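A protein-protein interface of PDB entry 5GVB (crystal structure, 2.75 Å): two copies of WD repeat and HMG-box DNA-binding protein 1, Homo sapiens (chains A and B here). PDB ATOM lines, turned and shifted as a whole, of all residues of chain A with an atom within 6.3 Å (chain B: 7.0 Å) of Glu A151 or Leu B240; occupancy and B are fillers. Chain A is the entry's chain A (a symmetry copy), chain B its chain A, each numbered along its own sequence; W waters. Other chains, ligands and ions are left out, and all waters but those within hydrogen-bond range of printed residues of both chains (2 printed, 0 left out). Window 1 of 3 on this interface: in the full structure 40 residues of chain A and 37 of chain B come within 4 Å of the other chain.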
ATOM      1  N   LEU A 140      -5.019 -23.995  -7.531  1.00  0.00           N
ATOM      2  CA  LEU A 140      -5.157 -22.856  -8.423  1.00  0.00           C
ATOM      3  C   LEU A 140      -3.810 -22.160  -8.516  1.00  0.00           C
ATOM      4  O   LEU A 140      -3.249 -21.733  -7.492  1.00  0.00           O
ATOM      5  CB  LEU A 140      -6.227 -21.877  -7.949  1.00  0.00           C
ATOM      6  CG  LEU A 140      -6.518 -20.908  -9.096  1.00  0.00           C
ATOM      7  CD1 LEU A 140      -7.989 -20.899  -9.410  1.00  0.00           C
ATOM      8  CD2 LEU A 140      -6.008 -19.501  -8.813  1.00  0.00           C
ATOM      9  N   ARG A 141      -3.307 -22.051  -9.741  1.00  0.00           N
ATOM     10  CA  ARG A 141      -2.000 -21.492 -10.040  1.00  0.00           C
ATOM     11  C   ARG A 141      -2.193 -20.240 -10.881  1.00  0.00           C
ATOM     12  O   ARG A 141      -2.887 -20.275 -11.905  1.00  0.00           O
ATOM     13  CB  ARG A 141      -1.132 -22.519 -10.774  1.00  0.00           C
ATOM     14  CG  ARG A 141      -1.381 -23.957 -10.318  1.00  0.00           C
ATOM     15  CD  ARG A 141      -0.382 -24.935 -10.919  1.00  0.00           C
ATOM     16  NE  ARG A 141       0.951 -24.772 -10.350  1.00  0.00           N
ATOM     17  CZ  ARG A 141       1.542 -25.660  -9.558  1.00  0.00           C
ATOM     18  NH1 ARG A 141       0.925 -26.790  -9.240  1.00  0.00           N
ATOM     19  NH2 ARG A 141       2.757 -25.419  -9.090  1.00  0.00           N
ATOM     20  N   LEU A 142      -1.592 -19.139 -10.437  1.00  0.00           N
ATOM     21  CA  LEU A 142      -1.732 -17.839 -11.077  1.00  0.00           C
ATOM     22  C   LEU A 142      -0.454 -17.476 -11.822  1.00  0.00           C
ATOM     23  O   LEU A 142       0.652 -17.813 -11.386  1.00  0.00           O
ATOM     24  CB  LEU A 142      -2.061 -16.754 -10.048  1.00  0.00           C
ATOM     25  CG  LEU A 142      -3.488 -16.752  -9.495  1.00  0.00           C
ATOM     26  CD1 LEU A 142      -3.622 -15.755  -8.357  1.00  0.00           C
ATOM     27  CD2 LEU A 142      -4.481 -16.438 -10.601  1.00  0.00           C
ATOM     28  N   PHE A 143      -0.619 -16.784 -12.945  1.00  0.00           N
ATOM     29  CA  PHE A 143       0.491 -16.373 -13.787  1.00  0.00           C
ATOM     30  C   PHE A 143       0.230 -14.969 -14.305  1.00  0.00           C
ATOM     31  O   PHE A 143      -0.919 -14.561 -14.481  1.00  0.00           O
ATOM     32  CB  PHE A 143       0.690 -17.318 -14.984  1.00  0.00           C
ATOM     33  CG  PHE A 143       0.855 -18.763 -14.608  1.00  0.00           C
ATOM     34  CD1 PHE A 143      -0.250 -19.559 -14.351  1.00  0.00           C
ATOM     35  CD2 PHE A 143       2.115 -19.329 -14.528  1.00  0.00           C
ATOM     36  CE1 PHE A 143      -0.098 -20.889 -14.006  1.00  0.00           C
ATOM     37  CE2 PHE A 143       2.274 -20.658 -14.187  1.00  0.00           C
ATOM     38  CZ  PHE A 143       1.165 -21.440 -13.927  1.00  0.00           C
ATOM     39  N   GLN A 149       5.171 -16.872 -12.572  1.00  0.00           N
ATOM     40  CA  GLN A 149       4.337 -17.580 -11.612  1.00  0.00           C
ATOM     41  C   GLN A 149       4.039 -16.672 -10.426  1.00  0.00           C
ATOM     42  O   GLN A 149       4.943 -16.024  -9.890  1.00  0.00           O
ATOM     43  CB  GLN A 149       5.036 -18.852 -11.137  1.00  0.00           C
ATOM     44  CG  GLN A 149       5.373 -19.839 -12.236  1.00  0.00           C
ATOM     45  CD  GLN A 149       6.026 -21.095 -11.697  1.00  0.00           C
ATOM     46  OE1 GLN A 149       5.346 -22.055 -11.341  1.00  0.00           O
ATOM     47  NE2 GLN A 149       7.353 -21.094 -11.634  1.00  0.00           N
ATOM     48  N   LYS A 150       2.773 -16.618 -10.015  1.00  0.00           N
ATOM     49  CA  LYS A 150       2.367 -15.823  -8.870  1.00  0.00           C
ATOM     50  C   LYS A 150       1.812 -16.758  -7.790  1.00  0.00           C
ATOM     51  O   LYS A 150       2.255 -17.917  -7.685  1.00  0.00           O
ATOM     52  CB  LYS A 150       1.367 -14.761  -9.321  1.00  0.00           C
ATOM     53  CG  LYS A 150       1.877 -13.871 -10.439  1.00  0.00           C
ATOM     54  CD  LYS A 150       1.116 -12.556 -10.491  1.00  0.00           C
ATOM     55  CE  LYS A 150       1.400 -11.711  -9.256  1.00  0.00           C
ATOM     56  NZ  LYS A 150       0.577 -10.471  -9.214  1.00  0.00           N
ATOM     57  N   GLU A 151       0.892 -16.243  -6.972  1.00  0.00           N
ATOM     58  CA  GLU A 151       0.362 -17.007  -5.855  1.00  0.00           C
ATOM     59  C   GLU A 151      -0.275 -18.326  -6.286  1.00  0.00           C
ATOM     60  O   GLU A 151      -0.701 -18.507  -7.431  1.00  0.00           O
ATOM     61  CB  GLU A 151      -0.655 -16.169  -5.077  1.00  0.00           C
ATOM     62  CG  GLU A 151      -0.112 -14.851  -4.541  1.00  0.00           C
ATOM     63  CD  GLU A 151      -0.392 -13.681  -5.467  1.00  0.00           C
ATOM     64  OE1 GLU A 151      -0.542 -13.904  -6.686  1.00  0.00           O
ATOM     65  OE2 GLU A 151      -0.468 -12.536  -4.971  1.00  0.00           O
ATOM     66  N   VAL A 152      -0.323 -19.261  -5.342  1.00  0.00           N
ATOM     67  CA  VAL A 152      -0.946 -20.566  -5.520  1.00  0.00           C
ATOM     68  C   VAL A 152      -1.808 -20.827  -4.295  1.00  0.00           C
ATOM     69  O   VAL A 152      -1.410 -20.495  -3.173  1.00  0.00           O
ATOM     70  CB  VAL A 152       0.106 -21.685  -5.689  1.00  0.00           C
ATOM     71  CG1 VAL A 152      -0.565 -23.036  -5.896  1.00  0.00           C
ATOM     72  CG2 VAL A 152       1.060 -21.370  -6.833  1.00  0.00           C
ATOM     73  N   PHE A 153      -2.990 -21.409  -4.496  1.00  0.00           N
ATOM     74  CA  PHE A 153      -3.771 -21.785  -3.322  1.00  0.00           C
ATOM     75  C   PHE A 153      -4.616 -23.010  -3.631  1.00  0.00           C
ATOM     76  O   PHE A 153      -4.863 -23.340  -4.789  1.00  0.00           O
ATOM     77  CB  PHE A 153      -4.643 -20.624  -2.808  1.00  0.00           C
ATOM     78  CG  PHE A 153      -5.699 -20.162  -3.773  1.00  0.00           C
ATOM     79  CD1 PHE A 153      -5.436 -19.135  -4.662  1.00  0.00           C
ATOM     80  CD2 PHE A 153      -6.965 -20.727  -3.765  1.00  0.00           C
ATOM     81  CE1 PHE A 153      -6.407 -18.695  -5.538  1.00  0.00           C
ATOM     82  CE2 PHE A 153      -7.941 -20.292  -4.642  1.00  0.00           C
ATOM     83  CZ  PHE A 153      -7.660 -19.276  -5.532  1.00  0.00           C
ATOM     84  N   LEU A 190     -12.983 -13.988  -6.202  1.00  0.00           N
ATOM     85  CA  LEU A 190     -11.778 -13.321  -5.730  1.00  0.00           C
ATOM     86  C   LEU A 190     -11.491 -12.068  -6.548  1.00  0.00           C
ATOM     87  O   LEU A 190     -11.842 -11.982  -7.728  1.00  0.00           O
ATOM     88  CB  LEU A 190     -10.556 -14.246  -5.814  1.00  0.00           C
ATOM     89  CG  LEU A 190     -10.499 -15.492  -4.933  1.00  0.00           C
ATOM     90  CD1 LEU A 190      -9.908 -16.644  -5.718  1.00  0.00           C
ATOM     91  CD2 LEU A 190      -9.669 -15.210  -3.694  1.00  0.00           C
ATOM     92  N   LEU A 192      -8.055  -9.796  -7.458  1.00  0.00           N
ATOM     93  CA  LEU A 192      -6.612 -10.014  -7.450  1.00  0.00           C
ATOM     94  C   LEU A 192      -5.821  -8.736  -7.717  1.00  0.00           C
ATOM     95  O   LEU A 192      -4.784  -8.759  -8.381  1.00  0.00           O
ATOM     96  CB  LEU A 192      -6.232 -11.086  -8.469  1.00  0.00           C
ATOM     97  CG  LEU A 192      -6.953 -12.429  -8.343  1.00  0.00           C
ATOM     98  CD1 LEU A 192      -6.621 -13.322  -9.527  1.00  0.00           C
ATOM     99  CD2 LEU A 192      -6.579 -13.108  -7.036  1.00  0.00           C
ATOM    100  N   LYS A 196      -5.752  -7.925  -2.158  1.00  0.00           N
ATOM    101  CA  LYS A 196      -6.404  -9.194  -2.456  1.00  0.00           C
ATOM    102  C   LYS A 196      -7.655  -9.366  -1.604  1.00  0.00           C
ATOM    103  O   LYS A 196      -7.663  -9.043  -0.412  1.00  0.00           O
ATOM    104  CB  LYS A 196      -5.446 -10.359  -2.216  1.00  0.00           C
ATOM    105  CG  LYS A 196      -4.162 -10.302  -3.031  1.00  0.00           C
ATOM    106  CD  LYS A 196      -4.447 -10.279  -4.524  1.00  0.00           C
ATOM    107  CE  LYS A 196      -3.161 -10.388  -5.334  1.00  0.00           C
ATOM    108  NZ  LYS A 196      -2.178  -9.334  -4.964  1.00  0.00           N
ATOM    109  N   LYS A 197      -8.720  -9.873  -2.223  1.00  0.00           N
ATOM    110  CA  LYS A 197      -9.988 -10.074  -1.536  1.00  0.00           C
ATOM    111  C   LYS A 197     -10.618 -11.388  -1.972  1.00  0.00           C
ATOM    112  O   LYS A 197     -10.502 -11.787  -3.134  1.00  0.00           O
ATOM    113  CB  LYS A 197     -10.977  -8.931  -1.811  1.00  0.00           C
ATOM    114  CG  LYS A 197     -10.456  -7.535  -1.524  1.00  0.00           C
ATOM    115  CD  LYS A 197     -11.601  -6.535  -1.484  1.00  0.00           C
ATOM    116  CE  LYS A 197     -11.148  -5.138  -1.870  1.00  0.00           C
ATOM    117  NZ  LYS A 197     -10.790  -5.052  -3.312  1.00  0.00           N
ATOM    118  N   GLN A 198     -11.289 -12.051  -1.035  1.00  0.00           N
ATOM    119  CA  GLN A 198     -12.149 -13.195  -1.325  1.00  0.00           C
ATOM    120  C   GLN A 198     -13.585 -12.712  -1.140  1.00  0.00           C
ATOM    121  O   GLN A 198     -14.120 -12.718  -0.031  1.00  0.00           O
ATOM    122  CB  GLN A 198     -11.842 -14.392  -0.428  1.00  0.00           C
ATOM    123  CG  GLN A 198     -12.636 -15.638  -0.805  1.00  0.00           C
ATOM    124  CD  GLN A 198     -12.269 -16.855   0.022  1.00  0.00           C
ATOM    125  OE1 GLN A 198     -12.856 -17.926  -0.137  1.00  0.00           O
ATOM    126  NE2 GLN A 198     -11.300 -16.695   0.914  1.00  0.00           N
ATOM    127  N   ASN B 237      -3.465 -17.946   4.234  1.00  0.00           N
ATOM    128  CA  ASN B 237      -2.806 -16.892   3.464  1.00  0.00           C
ATOM    129  C   ASN B 237      -3.600 -15.600   3.652  1.00  0.00           C
ATOM    130  O   ASN B 237      -4.480 -15.271   2.853  1.00  0.00           O
ATOM    131  CB  ASN B 237      -2.701 -17.288   1.992  1.00  0.00           C
ATOM    132  CG  ASN B 237      -1.704 -16.440   1.228  1.00  0.00           C
ATOM    133  OD1 ASN B 237      -1.548 -15.249   1.496  1.00  0.00           O
ATOM    134  ND2 ASN B 237      -1.021 -17.054   0.269  1.00  0.00           N
ATOM    135  N   ARG B 238      -3.272 -14.859   4.716  1.00  0.00           N
ATOM    136  CA  ARG B 238      -4.002 -13.633   5.021  1.00  0.00           C
ATOM    137  C   ARG B 238      -3.827 -12.580   3.934  1.00  0.00           C
ATOM    138  O   ARG B 238      -4.714 -11.743   3.737  1.00  0.00           O
ATOM    139  CB  ARG B 238      -3.561 -13.071   6.374  1.00  0.00           C
ATOM    140  CG  ARG B 238      -3.405 -14.107   7.478  1.00  0.00           C
ATOM    141  CD  ARG B 238      -3.430 -13.428   8.840  1.00  0.00           C
ATOM    142  NE  ARG B 238      -3.138 -14.340   9.942  1.00  0.00           N
ATOM    143  CZ  ARG B 238      -4.043 -14.774  10.813  1.00  0.00           C
ATOM    144  NH1 ARG B 238      -5.308 -14.392  10.705  1.00  0.00           N
ATOM    145  NH2 ARG B 238      -3.685 -15.596  11.790  1.00  0.00           N
ATOM    146  N   GLY B 239      -2.701 -12.601   3.224  1.00  0.00           N
ATOM    147  CA  GLY B 239      -2.492 -11.684   2.123  1.00  0.00           C
ATOM    148  C   GLY B 239      -3.191 -12.051   0.836  1.00  0.00           C
ATOM    149  O   GLY B 239      -3.062 -11.328  -0.156  1.00  0.00           O
ATOM    150  N   LEU B 240      -3.934 -13.156   0.820  1.00  0.00           N
ATOM    151  CA  LEU B 240      -4.635 -13.637  -0.365  1.00  0.00           C
ATOM    152  C   LEU B 240      -6.087 -13.962  -0.029  1.00  0.00           C
ATOM    153  O   LEU B 240      -6.619 -15.010  -0.408  1.00  0.00           O
ATOM    154  CB  LEU B 240      -3.918 -14.850  -0.960  1.00  0.00           C
ATOM    155  CG  LEU B 240      -4.292 -15.320  -2.370  1.00  0.00           C
ATOM    156  CD1 LEU B 240      -4.007 -14.239  -3.400  1.00  0.00           C
ATOM    157  CD2 LEU B 240      -3.556 -16.606  -2.718  1.00  0.00           C
ATOM    158  N   GLY B 241      -6.749 -13.064   0.699  1.00  0.00           N
ATOM    159  CA  GLY B 241      -8.157 -13.236   1.002  1.00  0.00           C
ATOM    160  C   GLY B 241      -8.485 -14.371   1.943  1.00  0.00           C
ATOM    161  O   GLY B 241      -9.608 -14.880   1.911  1.00  0.00           O
ATOM    162  N   ASN B 242      -7.536 -14.778   2.788  1.00  0.00           N
ATOM    163  CA  ASN B 242      -7.717 -15.891   3.724  1.00  0.00           C
ATOM    164  C   ASN B 242      -8.017 -17.197   2.992  1.00  0.00           C
ATOM    165  O   ASN B 242      -8.833 -18.010   3.435  1.00  0.00           O
ATOM    166  CB  ASN B 242      -8.798 -15.580   4.762  1.00  0.00           C
ATOM    167  CG  ASN B 242      -8.304 -14.646   5.849  1.00  0.00           C
ATOM    168  OD1 ASN B 242      -7.151 -14.727   6.273  1.00  0.00           O
ATOM    169  ND2 ASN B 242      -9.174 -13.753   6.306  1.00  0.00           N
ATOM    170  N   THR B 243      -7.352 -17.397   1.857  1.00  0.00           N
ATOM    171  CA  THR B 243      -7.303 -18.701   1.217  1.00  0.00           C
ATOM    172  C   THR B 243      -6.270 -19.572   1.930  1.00  0.00           C
ATOM    173  O   THR B 243      -5.661 -19.172   2.925  1.00  0.00           O
ATOM    174  CB  THR B 243      -6.982 -18.555  -0.269  1.00  0.00           C
ATOM    175  OG1 THR B 243      -5.884 -17.648  -0.435  1.00  0.00           O
ATOM    176  CG2 THR B 243      -8.191 -18.022  -1.027  1.00  0.00           C
ATOM    177  N   TRP B 244      -6.058 -20.782   1.418  1.00  0.00           N
ATOM    178  CA  TRP B 244      -5.134 -21.732   2.024  1.00  0.00           C
ATOM    179  C   TRP B 244      -4.078 -22.121   1.001  1.00  0.00           C
ATOM    180  O   TRP B 244      -4.403 -22.692  -0.045  1.00  0.00           O
ATOM    181  CB  TRP B 244      -5.880 -22.962   2.543  1.00  0.00           C
ATOM    182  CG  TRP B 244      -6.896 -22.619   3.588  1.00  0.00           C
ATOM    183  CD1 TRP B 244      -8.209 -22.311   3.385  1.00  0.00           C
ATOM    184  CD2 TRP B 244      -6.677 -22.528   5.002  1.00  0.00           C
ATOM    185  NE1 TRP B 244      -8.825 -22.044   4.585  1.00  0.00           N
ATOM    186  CE2 TRP B 244      -7.905 -22.169   5.593  1.00  0.00           C
ATOM    187  CE3 TRP B 244      -5.562 -22.720   5.826  1.00  0.00           C
ATOM    188  CZ2 TRP B 244      -8.051 -21.999   6.969  1.00  0.00           C
ATOM    189  CZ3 TRP B 244      -5.710 -22.549   7.192  1.00  0.00           C
ATOM    190  CH2 TRP B 244      -6.945 -22.193   7.749  1.00  0.00           C
ATOM    191  N   THR B 245      -2.816 -21.811   1.308  1.00  0.00           N
ATOM    192  CA  THR B 245      -1.698 -22.041   0.404  1.00  0.00           C
ATOM    193  C   THR B 245      -0.887 -23.240   0.863  1.00  0.00           C
ATOM    194  O   THR B 245      -0.517 -23.316   2.043  1.00  0.00           O
ATOM    195  CB  THR B 245      -0.800 -20.808   0.341  1.00  0.00           C
ATOM    196  OG1 THR B 245      -1.407 -19.809  -0.487  1.00  0.00           O
ATOM    197  CG2 THR B 245       0.573 -21.161  -0.221  1.00  0.00           C
ATOM    198  N   LEU B 299       7.108 -24.292  -1.555  1.00  0.00           N
ATOM    199  CA  LEU B 299       5.805 -24.160  -2.186  1.00  0.00           C
ATOM    200  C   LEU B 299       5.804 -24.894  -3.526  1.00  0.00           C
ATOM    201  O   LEU B 299       6.811 -24.890  -4.238  1.00  0.00           O
ATOM    202  CB  LEU B 299       5.449 -22.686  -2.387  1.00  0.00           C
ATOM    203  CG  LEU B 299       4.894 -21.899  -1.192  1.00  0.00           C
ATOM    204  CD1 LEU B 299       5.886 -21.812  -0.038  1.00  0.00           C
ATOM    205  CD2 LEU B 299       4.464 -20.506  -1.629  1.00  0.00           C
ATOM    206  N   TYR B 301       5.807 -25.017  -6.708  1.00  0.00           N
ATOM    207  CA  TYR B 301       5.901 -24.204  -7.910  1.00  0.00           C
ATOM    208  C   TYR B 301       6.435 -25.012  -9.085  1.00  0.00           C
ATOM    209  O   TYR B 301       7.127 -26.019  -8.914  1.00  0.00           O
ATOM    210  CB  TYR B 301       6.776 -22.975  -7.662  1.00  0.00           C
ATOM    211  CG  TYR B 301       5.971 -21.822  -7.121  1.00  0.00           C
ATOM    212  CD1 TYR B 301       5.584 -21.786  -5.789  1.00  0.00           C
ATOM    213  CD2 TYR B 301       5.562 -20.788  -7.952  1.00  0.00           C
ATOM    214  CE1 TYR B 301       4.830 -20.742  -5.294  1.00  0.00           C
ATOM    215  CE2 TYR B 301       4.809 -19.742  -7.467  1.00  0.00           C
ATOM    216  CZ  TYR B 301       4.446 -19.723  -6.138  1.00  0.00           C
ATOM    217  OH  TYR B 301       3.693 -18.682  -5.652  1.00  0.00           O
ATOM    218  N   TRP B 316       7.643 -15.990  -3.312  1.00  0.00           N
ATOM    219  CA  TRP B 316       6.314 -16.160  -2.738  1.00  0.00           C
ATOM    220  C   TRP B 316       6.372 -16.815  -1.362  1.00  0.00           C
ATOM    221  O   TRP B 316       5.522 -16.527  -0.502  1.00  0.00           O
ATOM    222  CB  TRP B 316       5.433 -16.941  -3.707  1.00  0.00           C
ATOM    223  CG  TRP B 316       5.161 -16.134  -4.938  1.00  0.00           C
ATOM    224  CD1 TRP B 316       5.597 -16.388  -6.206  1.00  0.00           C
ATOM    225  CD2 TRP B 316       4.432 -14.903  -5.005  1.00  0.00           C
ATOM    226  NE1 TRP B 316       5.162 -15.404  -7.062  1.00  0.00           N
ATOM    227  CE2 TRP B 316       4.446 -14.480  -6.348  1.00  0.00           C
ATOM    228  CE3 TRP B 316       3.757 -14.125  -4.059  1.00  0.00           C
ATOM    229  CZ2 TRP B 316       3.813 -13.312  -6.769  1.00  0.00           C
ATOM    230  CZ3 TRP B 316       3.129 -12.966  -4.478  1.00  0.00           C
ATOM    231  CH2 TRP B 316       3.161 -12.572  -5.822  1.00  0.00           C
ATOM    232  N   VAL B 319       6.954 -13.868   0.938  1.00  0.00           N
ATOM    233  CA  VAL B 319       5.720 -13.099   1.114  1.00  0.00           C
ATOM    234  C   VAL B 319       4.805 -13.772   2.134  1.00  0.00           C
ATOM    235  O   VAL B 319       4.419 -13.175   3.158  1.00  0.00           O
ATOM    236  CB  VAL B 319       5.011 -12.914  -0.240  1.00  0.00           C
ATOM    237  CG1 VAL B 319       3.605 -12.367  -0.040  1.00  0.00           C
ATOM    238  CG2 VAL B 319       5.823 -11.999  -1.148  1.00  0.00           C
ATOM    239  N   ASN B 323       3.463 -12.412   6.023  1.00  0.00           N
ATOM    240  CA  ASN B 323       2.137 -11.878   6.364  1.00  0.00           C
ATOM    241  C   ASN B 323       1.902 -11.770   7.878  1.00  0.00           C
ATOM    242  O   ASN B 323       1.191 -10.858   8.347  1.00  0.00           O
ATOM    243  CB  ASN B 323       1.043 -12.751   5.744  1.00  0.00           C
ATOM    244  CG  ASN B 323       1.003 -12.658   4.234  1.00  0.00           C
ATOM    245  OD1 ASN B 323       1.269 -11.604   3.658  1.00  0.00           O
ATOM    246  ND2 ASN B 323       0.663 -13.765   3.582  1.00  0.00           N
ATOM    247  N   LEU B 373       5.847  -5.253  -9.148  1.00  0.00           N
ATOM    248  CA  LEU B 373       5.916  -5.756  -7.783  1.00  0.00           C
ATOM    249  C   LEU B 373       7.010  -5.097  -6.952  1.00  0.00           C
ATOM    250  O   LEU B 373       7.138  -5.411  -5.764  1.00  0.00           O
ATOM    251  CB  LEU B 373       6.142  -7.271  -7.797  1.00  0.00           C
ATOM    252  CG  LEU B 373       4.966  -8.159  -8.199  1.00  0.00           C
ATOM    253  CD1 LEU B 373       5.431  -9.594  -8.380  1.00  0.00           C
ATOM    254  CD2 LEU B 373       3.870  -8.082  -7.152  1.00  0.00           C
HETATM  255  O   HOH W   1      -3.653  -8.278  -0.133  1.00  0.00           O
HETATM  256  O   HOH W   2      -6.011 -10.516   1.596  1.00  0.00           O
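The backbone NH (N) of Leu A142 is in hydrogen-bond range of the backbone carbonyl oxygen (O) of Glu A151 (3.2 Å). OG1 of Thr B245 sits at hydrogen-bond distance from ND2 of Asn B237, 2.9 Å away. O of Phe A153 is in hydrogen-bond range of N of Leu A140 (2.8 Å). The side-chain amide oxygen (OD1) of Asn B237 lies close to the backbone NH (N) of Gly B239 (3.4 Å). The backbone carbonyl oxygen (O) of Leu B240 lies within hydrogen-bond range of the side-chain hydroxyl (OG1) of Thr B243, 2.7 Å away. The backbone carbonyl oxygen (O) of Leu A142 lies within hydrogen-bond range of the backbone NH (N) of Lys A150 (2.8 Å).
Of chain B, only Leu B240 (3.8 Å), Tyr B301 (3.7 Å) and Trp B316 (3.7 Å) come within 4 Å of Glu A151. Of the printed residues of chain A, Gly B241 touches Gln A198 (2.7 Å). Of the printed residues of chain A, Asn B242 touches Gln A198 (3.8 Å). Of the printed residues of chain B, Phe A153 touches Leu B240 and Trp B244. Of the printed residues of chain A, Tyr B301 touches Arg A141 (3.6 Å), Gln A149 (3.6 Å), Lys A150 (2.6 Å), Glu A151 (3.7 Å) and Val A152 (3.8 Å). Of the printed residues of chain B, Lys A196 touches Gly B239 and Leu B240. The nearest residue of chain B that does not touch Glu A151 is Asn B237 (5.4 Å). The nearest printed residue of chain A that does not touch Asn B242 is Lys A196 (6.6 Å).
Water W2 lies within hydrogen-bond range of O of Arg B238, N of Gly B241, O of Lys A196 and N of Leu B240. Water W1 bridges the backbone NH of Lys A196 (2.9 Å) and the backbone carbonyl oxygen of Gly B239 (3.1 Å).
Among the printed residues, 17 pairs touch across the chains.
Among the printed residues, pairs that only touch across the chains: Lys A196 with Gly B239 (3.2 Å), Lys A150 with Trp B316 (3.4 Å), Phe A153 with Trp B244 (3.5 Å), Arg A141 with Tyr B301 (3.6 Å), Gln A149 with Tyr B301 (3.6 Å), Glu A151 with Trp B316 (3.7 Å), Phe A153 with Leu B240 (3.7 Å), Glu A151 with Tyr B301 (3.7 Å), Gln A198 with Asn B242 (3.8 Å), Glu A151 with Leu B240 (3.8 Å), Val A152 with Tyr B301 (3.8 Å), Lys A196 with Leu B240 (3.9 Å) and Gln A198 with Thr B243 (3.9 Å).
The indole nitrogen of Trp B316 sits at hydrogen-bond distance from the backbone carbonyl oxygen of Gln A149, 2.9 Å away. The backbone carbonyl oxygen (O) of Val A152 is in hydrogen-bond range of the side-chain hydroxyl (OG1) of Thr B245 (2.8 Å). The backbone carbonyl oxygen of Lys A150 lies within hydrogen-bond range of the side-chain hydroxyl of Tyr B301, 2.6 Å away. O of Gly B241 is in hydrogen-bond range of NE2 of Gln A198 (2.7 Å).
No position is printed for both chains. Of the 17 pairs that touch across the chains among the printed residues, none has its exchanged pair printed and touching as well.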
